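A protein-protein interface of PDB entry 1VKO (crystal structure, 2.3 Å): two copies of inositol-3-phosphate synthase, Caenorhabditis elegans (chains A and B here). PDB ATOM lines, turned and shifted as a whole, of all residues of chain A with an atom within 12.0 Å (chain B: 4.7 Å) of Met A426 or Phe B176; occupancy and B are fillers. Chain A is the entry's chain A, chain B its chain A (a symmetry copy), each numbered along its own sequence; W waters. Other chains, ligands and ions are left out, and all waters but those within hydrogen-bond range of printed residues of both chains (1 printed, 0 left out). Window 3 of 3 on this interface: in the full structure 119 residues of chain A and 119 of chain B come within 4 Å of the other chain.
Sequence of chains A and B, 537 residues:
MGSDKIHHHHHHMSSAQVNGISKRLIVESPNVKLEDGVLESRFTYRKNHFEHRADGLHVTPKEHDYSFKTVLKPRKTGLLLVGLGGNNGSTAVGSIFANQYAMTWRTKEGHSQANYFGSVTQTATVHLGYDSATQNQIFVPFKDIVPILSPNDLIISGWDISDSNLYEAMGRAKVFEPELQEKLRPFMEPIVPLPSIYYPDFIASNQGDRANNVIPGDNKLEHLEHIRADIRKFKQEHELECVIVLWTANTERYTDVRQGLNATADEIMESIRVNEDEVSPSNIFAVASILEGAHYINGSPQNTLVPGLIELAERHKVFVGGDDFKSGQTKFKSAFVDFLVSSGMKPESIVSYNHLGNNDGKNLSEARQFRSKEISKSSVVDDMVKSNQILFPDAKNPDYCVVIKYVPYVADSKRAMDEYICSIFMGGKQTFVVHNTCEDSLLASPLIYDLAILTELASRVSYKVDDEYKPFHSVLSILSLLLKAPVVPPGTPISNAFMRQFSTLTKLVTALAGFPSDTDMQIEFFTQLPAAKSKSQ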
ATOM      1  N   SER A 343     -32.448 -28.547 -26.408  1.00  0.00           N
ATOM      2  CA  SER A 343     -32.717 -28.642 -24.972  1.00  0.00           C
ATOM      3  C   SER A 343     -31.648 -27.999 -24.063  1.00  0.00           C
ATOM      4  O   SER A 343     -31.758 -28.092 -22.837  1.00  0.00           O
ATOM      5  CB  SER A 343     -32.903 -30.116 -24.541  1.00  0.00           C
ATOM      6  OG  SER A 343     -33.621 -30.916 -25.477  1.00  0.00           O
ATOM      7  N   GLY A 344     -30.609 -27.384 -24.632  1.00  0.00           N
ATOM      8  CA  GLY A 344     -29.554 -26.751 -23.820  1.00  0.00           C
ATOM      9  C   GLY A 344     -28.456 -27.638 -23.224  1.00  0.00           C
ATOM     10  O   GLY A 344     -27.896 -27.334 -22.120  1.00  0.00           O
ATOM     11  N   MET A 345     -28.120 -28.685 -23.983  1.00  0.00           N
ATOM     12  CA  MET A 345     -27.236 -29.802 -23.600  1.00  0.00           C
ATOM     13  C   MET A 345     -26.020 -29.904 -24.528  1.00  0.00           C
ATOM     14  O   MET A 345     -26.178 -29.921 -25.750  1.00  0.00           O
ATOM     15  CB  MET A 345     -28.011 -31.132 -23.737  1.00  0.00           C
ATOM     16  CG  MET A 345     -28.270 -31.897 -22.464  1.00  0.00           C
ATOM     17  SD  MET A 345     -29.919 -31.782 -21.741  1.00  0.00           S
ATOM     18  CE  MET A 345     -30.810 -32.850 -22.883  1.00  0.00           C
ATOM     19  N   LYS A 346     -24.824 -30.049 -23.957  1.00  0.00           N
ATOM     20  CA  LYS A 346     -23.562 -30.167 -24.738  1.00  0.00           C
ATOM     21  C   LYS A 346     -23.130 -31.617 -24.962  1.00  0.00           C
ATOM     22  O   LYS A 346     -22.580 -32.225 -24.054  1.00  0.00           O
ATOM     23  CB  LYS A 346     -22.428 -29.431 -24.018  1.00  0.00           C
ATOM     24  CG  LYS A 346     -21.233 -29.050 -24.885  1.00  0.00           C
ATOM     25  CD  LYS A 346     -20.142 -28.415 -24.001  1.00  0.00           C
ATOM     26  CE  LYS A 346     -18.815 -28.244 -24.758  1.00  0.00           C
ATOM     27  NZ  LYS A 346     -18.497 -29.468 -25.595  1.00  0.00           N
ATOM     28  N   GLU A 348     -20.623 -34.283 -25.674  1.00  0.00           N
ATOM     29  CA  GLU A 348     -19.193 -34.250 -25.366  1.00  0.00           C
ATOM     30  C   GLU A 348     -18.426 -35.367 -26.094  1.00  0.00           C
ATOM     31  O   GLU A 348     -17.216 -35.254 -26.377  1.00  0.00           O
ATOM     32  CB  GLU A 348     -18.991 -34.418 -23.858  1.00  0.00           C
ATOM     33  CG  GLU A 348     -19.597 -33.328 -23.006  1.00  0.00           C
ATOM     34  CD  GLU A 348     -18.747 -32.072 -22.959  1.00  0.00           C
ATOM     35  OE1 GLU A 348     -18.124 -31.693 -23.975  1.00  0.00           O
ATOM     36  OE2 GLU A 348     -18.708 -31.461 -21.890  1.00  0.00           O
ATOM     37  N   ILE A 390     -23.151 -20.721 -26.874  1.00  0.00           N
ATOM     38  CA  ILE A 390     -23.162 -20.793 -25.404  1.00  0.00           C
ATOM     39  C   ILE A 390     -22.592 -22.163 -25.023  1.00  0.00           C
ATOM     40  O   ILE A 390     -21.596 -22.256 -24.292  1.00  0.00           O
ATOM     41  CB  ILE A 390     -24.596 -20.567 -24.788  1.00  0.00           C
ATOM     42  CG1 ILE A 390     -25.155 -19.166 -25.131  1.00  0.00           C
ATOM     43  CG2 ILE A 390     -24.591 -20.807 -23.248  1.00  0.00           C
ATOM     44  CD1 ILE A 390     -26.692 -19.064 -25.057  1.00  0.00           C
ATOM     45  N   LEU A 391     -23.220 -23.211 -25.552  1.00  0.00           N
ATOM     46  CA  LEU A 391     -22.788 -24.594 -25.369  1.00  0.00           C
ATOM     47  C   LEU A 391     -21.378 -24.811 -25.910  1.00  0.00           C
ATOM     48  O   LEU A 391     -20.500 -25.332 -25.200  1.00  0.00           O
ATOM     49  CB  LEU A 391     -23.771 -25.545 -26.067  1.00  0.00           C
ATOM     50  CG  LEU A 391     -25.136 -25.744 -25.388  1.00  0.00           C
ATOM     51  CD1 LEU A 391     -26.041 -26.621 -26.227  1.00  0.00           C
ATOM     52  CD2 LEU A 391     -24.978 -26.346 -23.993  1.00  0.00           C
ATOM     53  N   CYS A 422     -23.261 -36.359 -22.671  1.00  0.00           N
ATOM     54  CA  CYS A 422     -23.509 -34.936 -22.713  1.00  0.00           C
ATOM     55  C   CYS A 422     -23.144 -34.371 -21.391  1.00  0.00           C
ATOM     56  O   CYS A 422     -23.229 -35.054 -20.380  1.00  0.00           O
ATOM     57  CB  CYS A 422     -24.993 -34.644 -22.975  1.00  0.00           C
ATOM     58  SG  CYS A 422     -25.482 -35.157 -24.619  1.00  0.00           S
ATOM     59  N   SER A 423     -22.734 -33.111 -21.408  1.00  0.00           N
ATOM     60  CA  SER A 423     -22.661 -32.307 -20.189  1.00  0.00           C
ATOM     61  C   SER A 423     -23.952 -31.467 -20.073  1.00  0.00           C
ATOM     62  O   SER A 423     -24.443 -30.867 -21.045  1.00  0.00           O
ATOM     63  CB  SER A 423     -21.387 -31.453 -20.162  1.00  0.00           C
ATOM     64  OG  SER A 423     -21.166 -30.857 -21.430  1.00  0.00           O
ATOM     65  N   ILE A 424     -24.523 -31.491 -18.876  1.00  0.00           N
ATOM     66  CA  ILE A 424     -25.799 -30.834 -18.568  1.00  0.00           C
ATOM     67  C   ILE A 424     -25.553 -29.787 -17.455  1.00  0.00           C
ATOM     68  O   ILE A 424     -24.415 -29.390 -17.234  1.00  0.00           O
ATOM     69  CB  ILE A 424     -26.878 -31.932 -18.190  1.00  0.00           C
ATOM     70  CG1 ILE A 424     -26.440 -32.777 -16.978  1.00  0.00           C
ATOM     71  CG2 ILE A 424     -27.176 -32.895 -19.429  1.00  0.00           C
ATOM     72  CD1 ILE A 424     -27.562 -33.600 -16.312  1.00  0.00           C
ATOM     73  N   PHE A 425     -26.611 -29.351 -16.776  1.00  0.00           N
ATOM     74  CA  PHE A 425     -26.551 -28.450 -15.627  1.00  0.00           C
ATOM     75  C   PHE A 425     -25.423 -28.719 -14.587  1.00  0.00           C
ATOM     76  O   PHE A 425     -25.277 -29.840 -14.063  1.00  0.00           O
ATOM     77  CB  PHE A 425     -27.920 -28.488 -14.929  1.00  0.00           C
ATOM     78  CG  PHE A 425     -28.150 -27.352 -13.928  1.00  0.00           C
ATOM     79  CD1 PHE A 425     -28.102 -26.023 -14.332  1.00  0.00           C
ATOM     80  CD2 PHE A 425     -28.470 -27.629 -12.600  1.00  0.00           C
ATOM     81  CE1 PHE A 425     -28.336 -24.977 -13.417  1.00  0.00           C
ATOM     82  CE2 PHE A 425     -28.727 -26.591 -11.682  1.00  0.00           C
ATOM     83  CZ  PHE A 425     -28.655 -25.265 -12.102  1.00  0.00           C
ATOM     84  N   MET A 426     -24.646 -27.678 -14.283  1.00  0.00           N
ATOM     85  CA  MET A 426     -23.662 -27.707 -13.182  1.00  0.00           C
ATOM     86  C   MET A 426     -22.637 -28.840 -13.302  1.00  0.00           C
ATOM     87  O   MET A 426     -22.294 -29.492 -12.283  1.00  0.00           O
ATOM     88  CB  MET A 426     -24.356 -27.802 -11.802  1.00  0.00           C
ATOM     89  CG  MET A 426     -25.155 -26.574 -11.351  1.00  0.00           C
ATOM     90  SD  MET A 426     -24.195 -25.156 -10.910  1.00  0.00           S
ATOM     91  CE  MET A 426     -23.447 -25.671  -9.398  1.00  0.00           C
ATOM     92  N   GLY A 427     -22.195 -29.100 -14.546  1.00  0.00           N
ATOM     93  CA  GLY A 427     -21.091 -30.042 -14.815  1.00  0.00           C
ATOM     94  C   GLY A 427     -21.469 -31.492 -14.540  1.00  0.00           C
ATOM     95  O   GLY A 427     -20.629 -32.411 -14.576  1.00  0.00           O
ATOM     96  N   GLY A 428     -22.750 -31.687 -14.234  1.00  0.00           N
ATOM     97  CA  GLY A 428     -23.344 -33.022 -14.267  1.00  0.00           C
ATOM     98  C   GLY A 428     -23.200 -33.621 -15.648  1.00  0.00           C
ATOM     99  O   GLY A 428     -22.906 -32.917 -16.628  1.00  0.00           O
ATOM    100  N   LYS A 429     -23.386 -34.940 -15.713  1.00  0.00           N
ATOM    101  CA  LYS A 429     -23.329 -35.674 -16.966  1.00  0.00           C
ATOM    102  C   LYS A 429     -24.610 -36.477 -17.180  1.00  0.00           C
ATOM    103  O   LYS A 429     -25.247 -36.937 -16.219  1.00  0.00           O
ATOM    104  CB  LYS A 429     -22.103 -36.598 -16.910  1.00  0.00           C
ATOM    105  CG  LYS A 429     -21.099 -36.421 -18.063  1.00  0.00           C
ATOM    106  CD  LYS A 429     -20.548 -34.986 -18.198  1.00  0.00           C
ATOM    107  CE  LYS A 429     -19.747 -34.528 -16.977  1.00  0.00           C
ATOM    108  NZ  LYS A 429     -18.573 -35.412 -16.773  1.00  0.00           N
ATOM    109  N   GLN A 430     -24.966 -36.656 -18.458  1.00  0.00           N
ATOM    110  CA  GLN A 430     -26.037 -37.541 -18.903  1.00  0.00           C
ATOM    111  C   GLN A 430     -25.539 -38.484 -20.019  1.00  0.00           C
ATOM    112  O   GLN A 430     -25.071 -38.047 -21.067  1.00  0.00           O
ATOM    113  CB  GLN A 430     -27.223 -36.744 -19.415  1.00  0.00           C
ATOM    114  CG  GLN A 430     -28.410 -37.610 -19.769  1.00  0.00           C
ATOM    115  CD  GLN A 430     -29.692 -36.821 -19.997  1.00  0.00           C
ATOM    116  OE1 GLN A 430     -29.657 -35.617 -20.353  1.00  0.00           O
ATOM    117  NE2 GLN A 430     -30.839 -37.501 -19.802  1.00  0.00           N
ATOM    118  N   SER B  90     -33.368 -27.682  -2.948  1.00  0.00           N
ATOM    119  CA  SER B  90     -32.094 -27.215  -2.370  1.00  0.00           C
ATOM    120  C   SER B  90     -31.068 -27.032  -3.495  1.00  0.00           C
ATOM    121  O   SER B  90     -30.171 -26.198  -3.425  1.00  0.00           O
ATOM    122  CB  SER B  90     -31.574 -28.200  -1.329  1.00  0.00           C
ATOM    123  OG  SER B  90     -31.359 -29.479  -1.920  1.00  0.00           O
ATOM    124  N   THR B  91     -31.225 -27.808  -4.558  1.00  0.00           N
ATOM    125  CA  THR B  91     -30.342 -27.691  -5.707  1.00  0.00           C
ATOM    126  C   THR B  91     -30.623 -26.441  -6.524  1.00  0.00           C
ATOM    127  O   THR B  91     -29.686 -25.773  -6.948  1.00  0.00           O
ATOM    128  CB  THR B  91     -30.453 -28.953  -6.588  1.00  0.00           C
ATOM    129  OG1 THR B  91     -29.907 -30.059  -5.865  1.00  0.00           O
ATOM    130  CG2 THR B  91     -29.559 -28.833  -7.812  1.00  0.00           C
ATOM    131  N   GLY B  94     -29.160 -23.758  -4.430  1.00  0.00           N
ATOM    132  CA  GLY B  94     -27.710 -23.900  -4.442  1.00  0.00           C
ATOM    133  C   GLY B  94     -27.054 -23.385  -5.703  1.00  0.00           C
ATOM    134  O   GLY B  94     -26.101 -22.600  -5.646  1.00  0.00           O
ATOM    135  N   SER B  95     -27.568 -23.830  -6.849  1.00  0.00           N
ATOM    136  CA  SER B  95     -27.021 -23.482  -8.153  1.00  0.00           C
ATOM    137  C   SER B  95     -27.134 -22.011  -8.535  1.00  0.00           C
ATOM    138  O   SER B  95     -26.267 -21.505  -9.273  1.00  0.00           O
ATOM    139  CB  SER B  95     -27.647 -24.342  -9.247  1.00  0.00           C
ATOM    140  OG  SER B  95     -27.510 -25.720  -8.951  1.00  0.00           O
ATOM    141  N   ALA B  98     -24.374 -20.525  -6.669  1.00  0.00           N
ATOM    142  CA  ALA B  98     -23.170 -21.043  -7.236  1.00  0.00           C
ATOM    143  C   ALA B  98     -22.862 -20.295  -8.505  1.00  0.00           C
ATOM    144  O   ALA B  98     -21.710 -19.944  -8.739  1.00  0.00           O
ATOM    145  CB  ALA B  98     -23.318 -22.519  -7.485  1.00  0.00           C
ATOM    146  N   ASN B  99     -23.876 -20.030  -9.330  1.00  0.00           N
ATOM    147  CA  ASN B  99     -23.663 -19.179 -10.528  1.00  0.00           C
ATOM    148  C   ASN B  99     -23.404 -17.686 -10.248  1.00  0.00           C
ATOM    149  O   ASN B  99     -22.651 -17.047 -10.972  1.00  0.00           O
ATOM    150  CB  ASN B  99     -24.793 -19.332 -11.539  1.00  0.00           C
ATOM    151  CG  ASN B  99     -24.693 -20.610 -12.314  1.00  0.00           C
ATOM    152  OD1 ASN B  99     -24.193 -20.631 -13.450  1.00  0.00           O
ATOM    153  ND2 ASN B  99     -25.170 -21.700 -11.712  1.00  0.00           N
ATOM    154  N   TRP B 105     -15.152 -26.269  -8.621  1.00  0.00           N
ATOM    155  CA  TRP B 105     -14.732 -27.345  -7.719  1.00  0.00           C
ATOM    156  C   TRP B 105     -13.721 -28.234  -8.447  1.00  0.00           C
ATOM    157  O   TRP B 105     -13.776 -28.328  -9.680  1.00  0.00           O
ATOM    158  CB  TRP B 105     -15.952 -28.123  -7.165  1.00  0.00           C
ATOM    159  CG  TRP B 105     -16.897 -28.626  -8.213  1.00  0.00           C
ATOM    160  CD1 TRP B 105     -16.945 -29.883  -8.707  1.00  0.00           C
ATOM    161  CD2 TRP B 105     -17.913 -27.873  -8.914  1.00  0.00           C
ATOM    162  NE1 TRP B 105     -17.919 -29.984  -9.672  1.00  0.00           N
ATOM    163  CE2 TRP B 105     -18.546 -28.772  -9.810  1.00  0.00           C
ATOM    164  CE3 TRP B 105     -18.356 -26.528  -8.871  1.00  0.00           C
ATOM    165  CZ2 TRP B 105     -19.586 -28.378 -10.690  1.00  0.00           C
ATOM    166  CZ3 TRP B 105     -19.407 -26.134  -9.708  1.00  0.00           C
ATOM    167  CH2 TRP B 105     -20.006 -27.072 -10.631  1.00  0.00           C
ATOM    168  N   ALA B 114     -19.672 -23.542 -11.984  1.00  0.00           N
ATOM    169  CA  ALA B 114     -21.129 -23.358 -12.043  1.00  0.00           C
ATOM    170  C   ALA B 114     -21.602 -22.977 -13.455  1.00  0.00           C
ATOM    171  O   ALA B 114     -20.917 -22.227 -14.169  1.00  0.00           O
ATOM    172  CB  ALA B 114     -21.568 -22.331 -11.056  1.00  0.00           C
ATOM    173  N   ASN B 115     -22.740 -23.534 -13.874  1.00  0.00           N
ATOM    174  CA  ASN B 115     -23.424 -23.035 -15.066  1.00  0.00           C
ATOM    175  C   ASN B 115     -24.934 -23.275 -15.036  1.00  0.00           C
ATOM    176  O   ASN B 115     -25.468 -23.711 -14.018  1.00  0.00           O
ATOM    177  CB  ASN B 115     -22.795 -23.591 -16.353  1.00  0.00           C
ATOM    178  CG  ASN B 115     -22.888 -25.107 -16.452  1.00  0.00           C
ATOM    179  OD1 ASN B 115     -23.808 -25.728 -15.920  1.00  0.00           O
ATOM    180  ND2 ASN B 115     -21.942 -25.706 -17.162  1.00  0.00           N
ATOM    181  N   MET B 170     -28.611 -30.203   1.390  1.00  0.00           N
ATOM    182  CA  MET B 170     -27.690 -30.566   0.320  1.00  0.00           C
ATOM    183  C   MET B 170     -26.990 -31.903   0.572  1.00  0.00           C
ATOM    184  O   MET B 170     -26.774 -32.714  -0.374  1.00  0.00           O
ATOM    185  CB  MET B 170     -26.617 -29.532   0.199  1.00  0.00           C
ATOM    186  CG  MET B 170     -27.018 -28.247  -0.431  1.00  0.00           C
ATOM    187  SD  MET B 170     -25.463 -27.387  -0.660  1.00  0.00           S
ATOM    188  CE  MET B 170     -26.050 -26.441  -2.021  1.00  0.00           C
ATOM    189  N   LYS B 174     -27.417 -35.191  -1.974  1.00  0.00           N
ATOM    190  CA  LYS B 174     -26.259 -35.901  -2.579  1.00  0.00           C
ATOM    191  C   LYS B 174     -26.098 -35.546  -4.057  1.00  0.00           C
ATOM    192  O   LYS B 174     -25.714 -36.397  -4.855  1.00  0.00           O
ATOM    193  CB  LYS B 174     -26.387 -37.438  -2.438  1.00  0.00           C
ATOM    194  CG  LYS B 174     -26.511 -37.936  -0.999  1.00  0.00           C
ATOM    195  CD  LYS B 174     -26.302 -39.421  -0.897  1.00  0.00           C
ATOM    196  CE  LYS B 174     -27.594 -40.231  -0.922  1.00  0.00           C
ATOM    197  NZ  LYS B 174     -28.317 -40.144   0.381  1.00  0.00           N
ATOM    198  N   VAL B 175     -26.415 -34.308  -4.413  1.00  0.00           N
ATOM    199  CA  VAL B 175     -26.282 -33.814  -5.784  1.00  0.00           C
ATOM    200  C   VAL B 175     -24.941 -33.104  -6.058  1.00  0.00           C
ATOM    201  O   VAL B 175     -24.203 -33.466  -6.990  1.00  0.00           O
ATOM    202  CB  VAL B 175     -27.478 -32.873  -6.125  1.00  0.00           C
ATOM    203  CG1 VAL B 175     -27.473 -32.479  -7.584  1.00  0.00           C
ATOM    204  CG2 VAL B 175     -28.797 -33.578  -5.793  1.00  0.00           C
ATOM    205  N   PHE B 176     -24.622 -32.083  -5.263  1.00  0.00           N
ATOM    206  CA  PHE B 176     -23.377 -31.366  -5.439  1.00  0.00           C
ATOM    207  C   PHE B 176     -22.256 -32.191  -4.819  1.00  0.00           C
ATOM    208  O   PHE B 176     -22.434 -32.831  -3.781  1.00  0.00           O
ATOM    209  CB  PHE B 176     -23.428 -30.020  -4.712  1.00  0.00           C
ATOM    210  CG  PHE B 176     -24.518 -29.098  -5.199  1.00  0.00           C
ATOM    211  CD1 PHE B 176     -24.490 -28.564  -6.470  1.00  0.00           C
ATOM    212  CD2 PHE B 176     -25.544 -28.736  -4.365  1.00  0.00           C
ATOM    213  CE1 PHE B 176     -25.505 -27.695  -6.913  1.00  0.00           C
ATOM    214  CE2 PHE B 176     -26.547 -27.858  -4.781  1.00  0.00           C
ATOM    215  CZ  PHE B 176     -26.520 -27.343  -6.074  1.00  0.00           C
ATOM    216  N   GLU B 177     -21.087 -32.136  -5.441  1.00  0.00           N
ATOM    217  CA  GLU B 177     -19.882 -32.785  -4.931  1.00  0.00           C
ATOM    218  C   GLU B 177     -19.526 -32.128  -3.565  1.00  0.00           C
ATOM    219  O   GLU B 177     -19.928 -30.993  -3.372  1.00  0.00           O
ATOM    220  CB  GLU B 177     -18.772 -32.528  -5.938  1.00  0.00           C
ATOM    221  CG  GLU B 177     -18.875 -33.275  -7.240  1.00  0.00           C
ATOM    222  CD  GLU B 177     -19.075 -34.765  -7.047  1.00  0.00           C
ATOM    223  OE1 GLU B 177     -18.278 -35.425  -6.347  1.00  0.00           O
ATOM    224  OE2 GLU B 177     -20.056 -35.255  -7.589  1.00  0.00           O
ATOM    225  N   PRO B 178     -18.823 -32.811  -2.647  1.00  0.00           N
ATOM    226  CA  PRO B 178     -18.630 -32.304  -1.296  1.00  0.00           C
ATOM    227  C   PRO B 178     -18.104 -30.892  -1.382  1.00  0.00           C
ATOM    228  O   PRO B 178     -18.772 -30.001  -0.922  1.00  0.00           O
ATOM    229  CB  PRO B 178     -17.608 -33.292  -0.693  1.00  0.00           C
ATOM    230  CG  PRO B 178     -18.075 -34.655  -1.437  1.00  0.00           C
ATOM    231  CD  PRO B 178     -18.145 -34.110  -2.812  1.00  0.00           C
ATOM    232  N   LEU B 180     -18.289 -28.444  -3.372  1.00  0.00           N
ATOM    233  CA  LEU B 180     -19.278 -27.396  -3.712  1.00  0.00           C
ATOM    234  C   LEU B 180     -20.323 -27.150  -2.622  1.00  0.00           C
ATOM    235  O   LEU B 180     -20.890 -26.055  -2.533  1.00  0.00           O
ATOM    236  CB  LEU B 180     -19.953 -27.666  -5.086  1.00  0.00           C
ATOM    237  CG  LEU B 180     -21.047 -26.712  -5.597  1.00  0.00           C
ATOM    238  CD1 LEU B 180     -20.564 -25.252  -5.692  1.00  0.00           C
ATOM    239  CD2 LEU B 180     -21.594 -27.227  -6.957  1.00  0.00           C
ATOM    240  N   GLN B 181     -20.585 -28.161  -1.798  1.00  0.00           N
ATOM    241  CA  GLN B 181     -21.498 -28.008  -0.666  1.00  0.00           C
ATOM    242  C   GLN B 181     -20.798 -27.158   0.387  1.00  0.00           C
ATOM    243  O   GLN B 181     -21.432 -26.302   1.031  1.00  0.00           O
ATOM    244  CB  GLN B 181     -21.894 -29.370  -0.071  1.00  0.00           C
ATOM    245  CG  GLN B 181     -22.779 -30.274  -0.976  1.00  0.00           C
ATOM    246  CD  GLN B 181     -23.147 -31.601  -0.325  1.00  0.00           C
ATOM    247  OE1 GLN B 181     -23.297 -31.662   0.909  1.00  0.00           O
ATOM    248  NE2 GLN B 181     -23.272 -32.684  -1.147  1.00  0.00           N
ATOM    249  N   LEU B 184     -20.851 -23.566  -0.733  1.00  0.00           N
ATOM    250  CA  LEU B 184     -22.226 -23.056  -0.604  1.00  0.00           C
ATOM    251  C   LEU B 184     -22.759 -22.956   0.827  1.00  0.00           C
ATOM    252  O   LEU B 184     -23.803 -22.338   1.063  1.00  0.00           O
ATOM    253  CB  LEU B 184     -23.173 -23.850  -1.449  1.00  0.00           C
ATOM    254  CG  LEU B 184     -23.124 -23.681  -2.962  1.00  0.00           C
ATOM    255  CD1 LEU B 184     -23.910 -24.786  -3.432  1.00  0.00           C
ATOM    256  CD2 LEU B 184     -23.781 -22.364  -3.377  1.00  0.00           C
ATOM    257  N   LEU B 442     -30.366 -32.500 -11.264  1.00  0.00           N
ATOM    258  CA  LEU B 442     -29.622 -31.728 -12.262  1.00  0.00           C
ATOM    259  C   LEU B 442     -30.442 -31.584 -13.558  1.00  0.00           C
ATOM    260  O   LEU B 442     -30.280 -30.632 -14.314  1.00  0.00           O
ATOM    261  CB  LEU B 442     -28.235 -32.349 -12.507  1.00  0.00           C
ATOM    262  CG  LEU B 442     -27.197 -32.294 -11.356  1.00  0.00           C
ATOM    263  CD1 LEU B 442     -25.891 -32.988 -11.762  1.00  0.00           C
ATOM    264  CD2 LEU B 442     -26.895 -30.862 -10.850  1.00  0.00           C
HETATM  265  O   HOH W   1     -29.739 -30.502 -17.139  1.00  0.00           O
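SD of Met A426 sits at hydrogen-bond distance from ND2 of Asn B99. The backbone NH of Met A426 is in hydrogen-bond range of the side-chain amide oxygen of Asn B115 (2.7 Å).
The side-chain hydroxyl of Ser B95 is in hydrogen-bond range of the backbone carbonyl oxygen of Thr B91 (3.0 Å). ND2 of Asn B99 is in hydrogen-bond range of O of Ser B95, 2.7 Å away. ND2 of Asn B99 lies within hydrogen-bond range of O of Asn B115. NE2 of Gln B181 sits at hydrogen-bond distance from O of Phe B176 (2.8 Å).
Ile A424 touches Asn B115. Phe A425 touches Asn B115 (CE1 to O, 3.2 Å). Phe A425 touches Leu B442 (CB to O, 3.2 Å). Met A426 touches Ser B95. Ala B98 touches Met A426. Met A426 touches Trp B105 (O to CZ2, 3.3 Å). Ala B114 touches Met A426. Phe B176 touches Met A426 (CE1 to CE, 3.8 Å). CE of Met A426 touches CD2 of Leu B180, 3.4 Å away. CA of Gly A428 touches CD1 of Leu B442 (3.6 Å).
Of chain B, only Ser B95 (3.5 Å), Ala B98 (3.7 Å), Asn B99 (3.7 Å), Trp B105 (3.3 Å), Ala B114 (3.7 Å), Asn B115 (2.7 Å), Phe B176 (3.8 Å) and Leu B180 (3.4 Å) come within 4 Å of Met A426. No residue of chain A comes within 4 Å of Ser B90. No residue of chain A comes within 4 Å of Gly B94. Ser B95 touches just these residues of chain A: Phe A425 (3.1 Å) and Met A426 (3.5 Å). Of chain A, only Met A426 (3.7 Å) comes within 4 Å of Ala B98. Printed residues of chain A within 4 Å of Ala B114: Met A426. No residue of chain A comes within 4 Å of Met B170. No residue of chain A comes within 4 Å of Val B175. No residue of chain A comes within 4 Å of Glu B177. No residue of chain A comes within 4 Å of Pro B178. Of chain A, only Met A426 (3.4 Å) comes within 4 Å of Leu B180. No residue of chain A comes within 4 Å of Gln B181. Of the printed residues of chain B, Ile A424 touches Asn B115 (3.9 Å). Printed residues of chain A within 4 Å of Asn B99: Met A426. Printed residues of chain A within 4 Å of Asn B115: Ile A424, Phe A425, Met A426 and Gly A427. Of the printed residues of chain A, Trp B105 touches Met A426. The nearest residue of chain B that does not touch Met A426 is Leu B442 (4.1 Å). The nearest printed residue of chain A that does not touch Asn B115 is Gly A428 (6.3 Å).
Of the 19 printed residues of chain B, 9 touch a printed residue of chain A. Printed residues of chain B that touch a printed residue of chain A: Ser B95, Ala B98, Asn B99, Trp B105, Ala B114, Asn B115, Phe B176, Leu B180 and Leu B442. Hydrophobic or aromatic side chains of chain B that line the printed part of chain A: Ala B98, Trp B105, Ala B114, Phe B176, Leu B180 and Leu B442. Along chain B the printed residues that touch a printed residue of chain A span positions 95 to 442. Of the 16 printed residues of chain A, 5 touch a printed residue of chain B. Hydrophobic or aromatic side chains of chain A within 4 Å of the printed part of chain B: Phe A425 and Met A426. Among the printed residues, no Asp or Glu carboxylate lies within 4 Å of a Lys or Arg side-chain nitrogen of the other chain.
No position is printed for both chains. Of the 14 pairs that touch across the chains among the printed residues, none has its exchanged pair printed and touching as well.
Water W1 lies within hydrogen-bond range of the backbone carbonyl oxygen (O) of Leu B442 (2.9 Å) and the backbone NH (N) of Phe A425 (3.4 Å).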
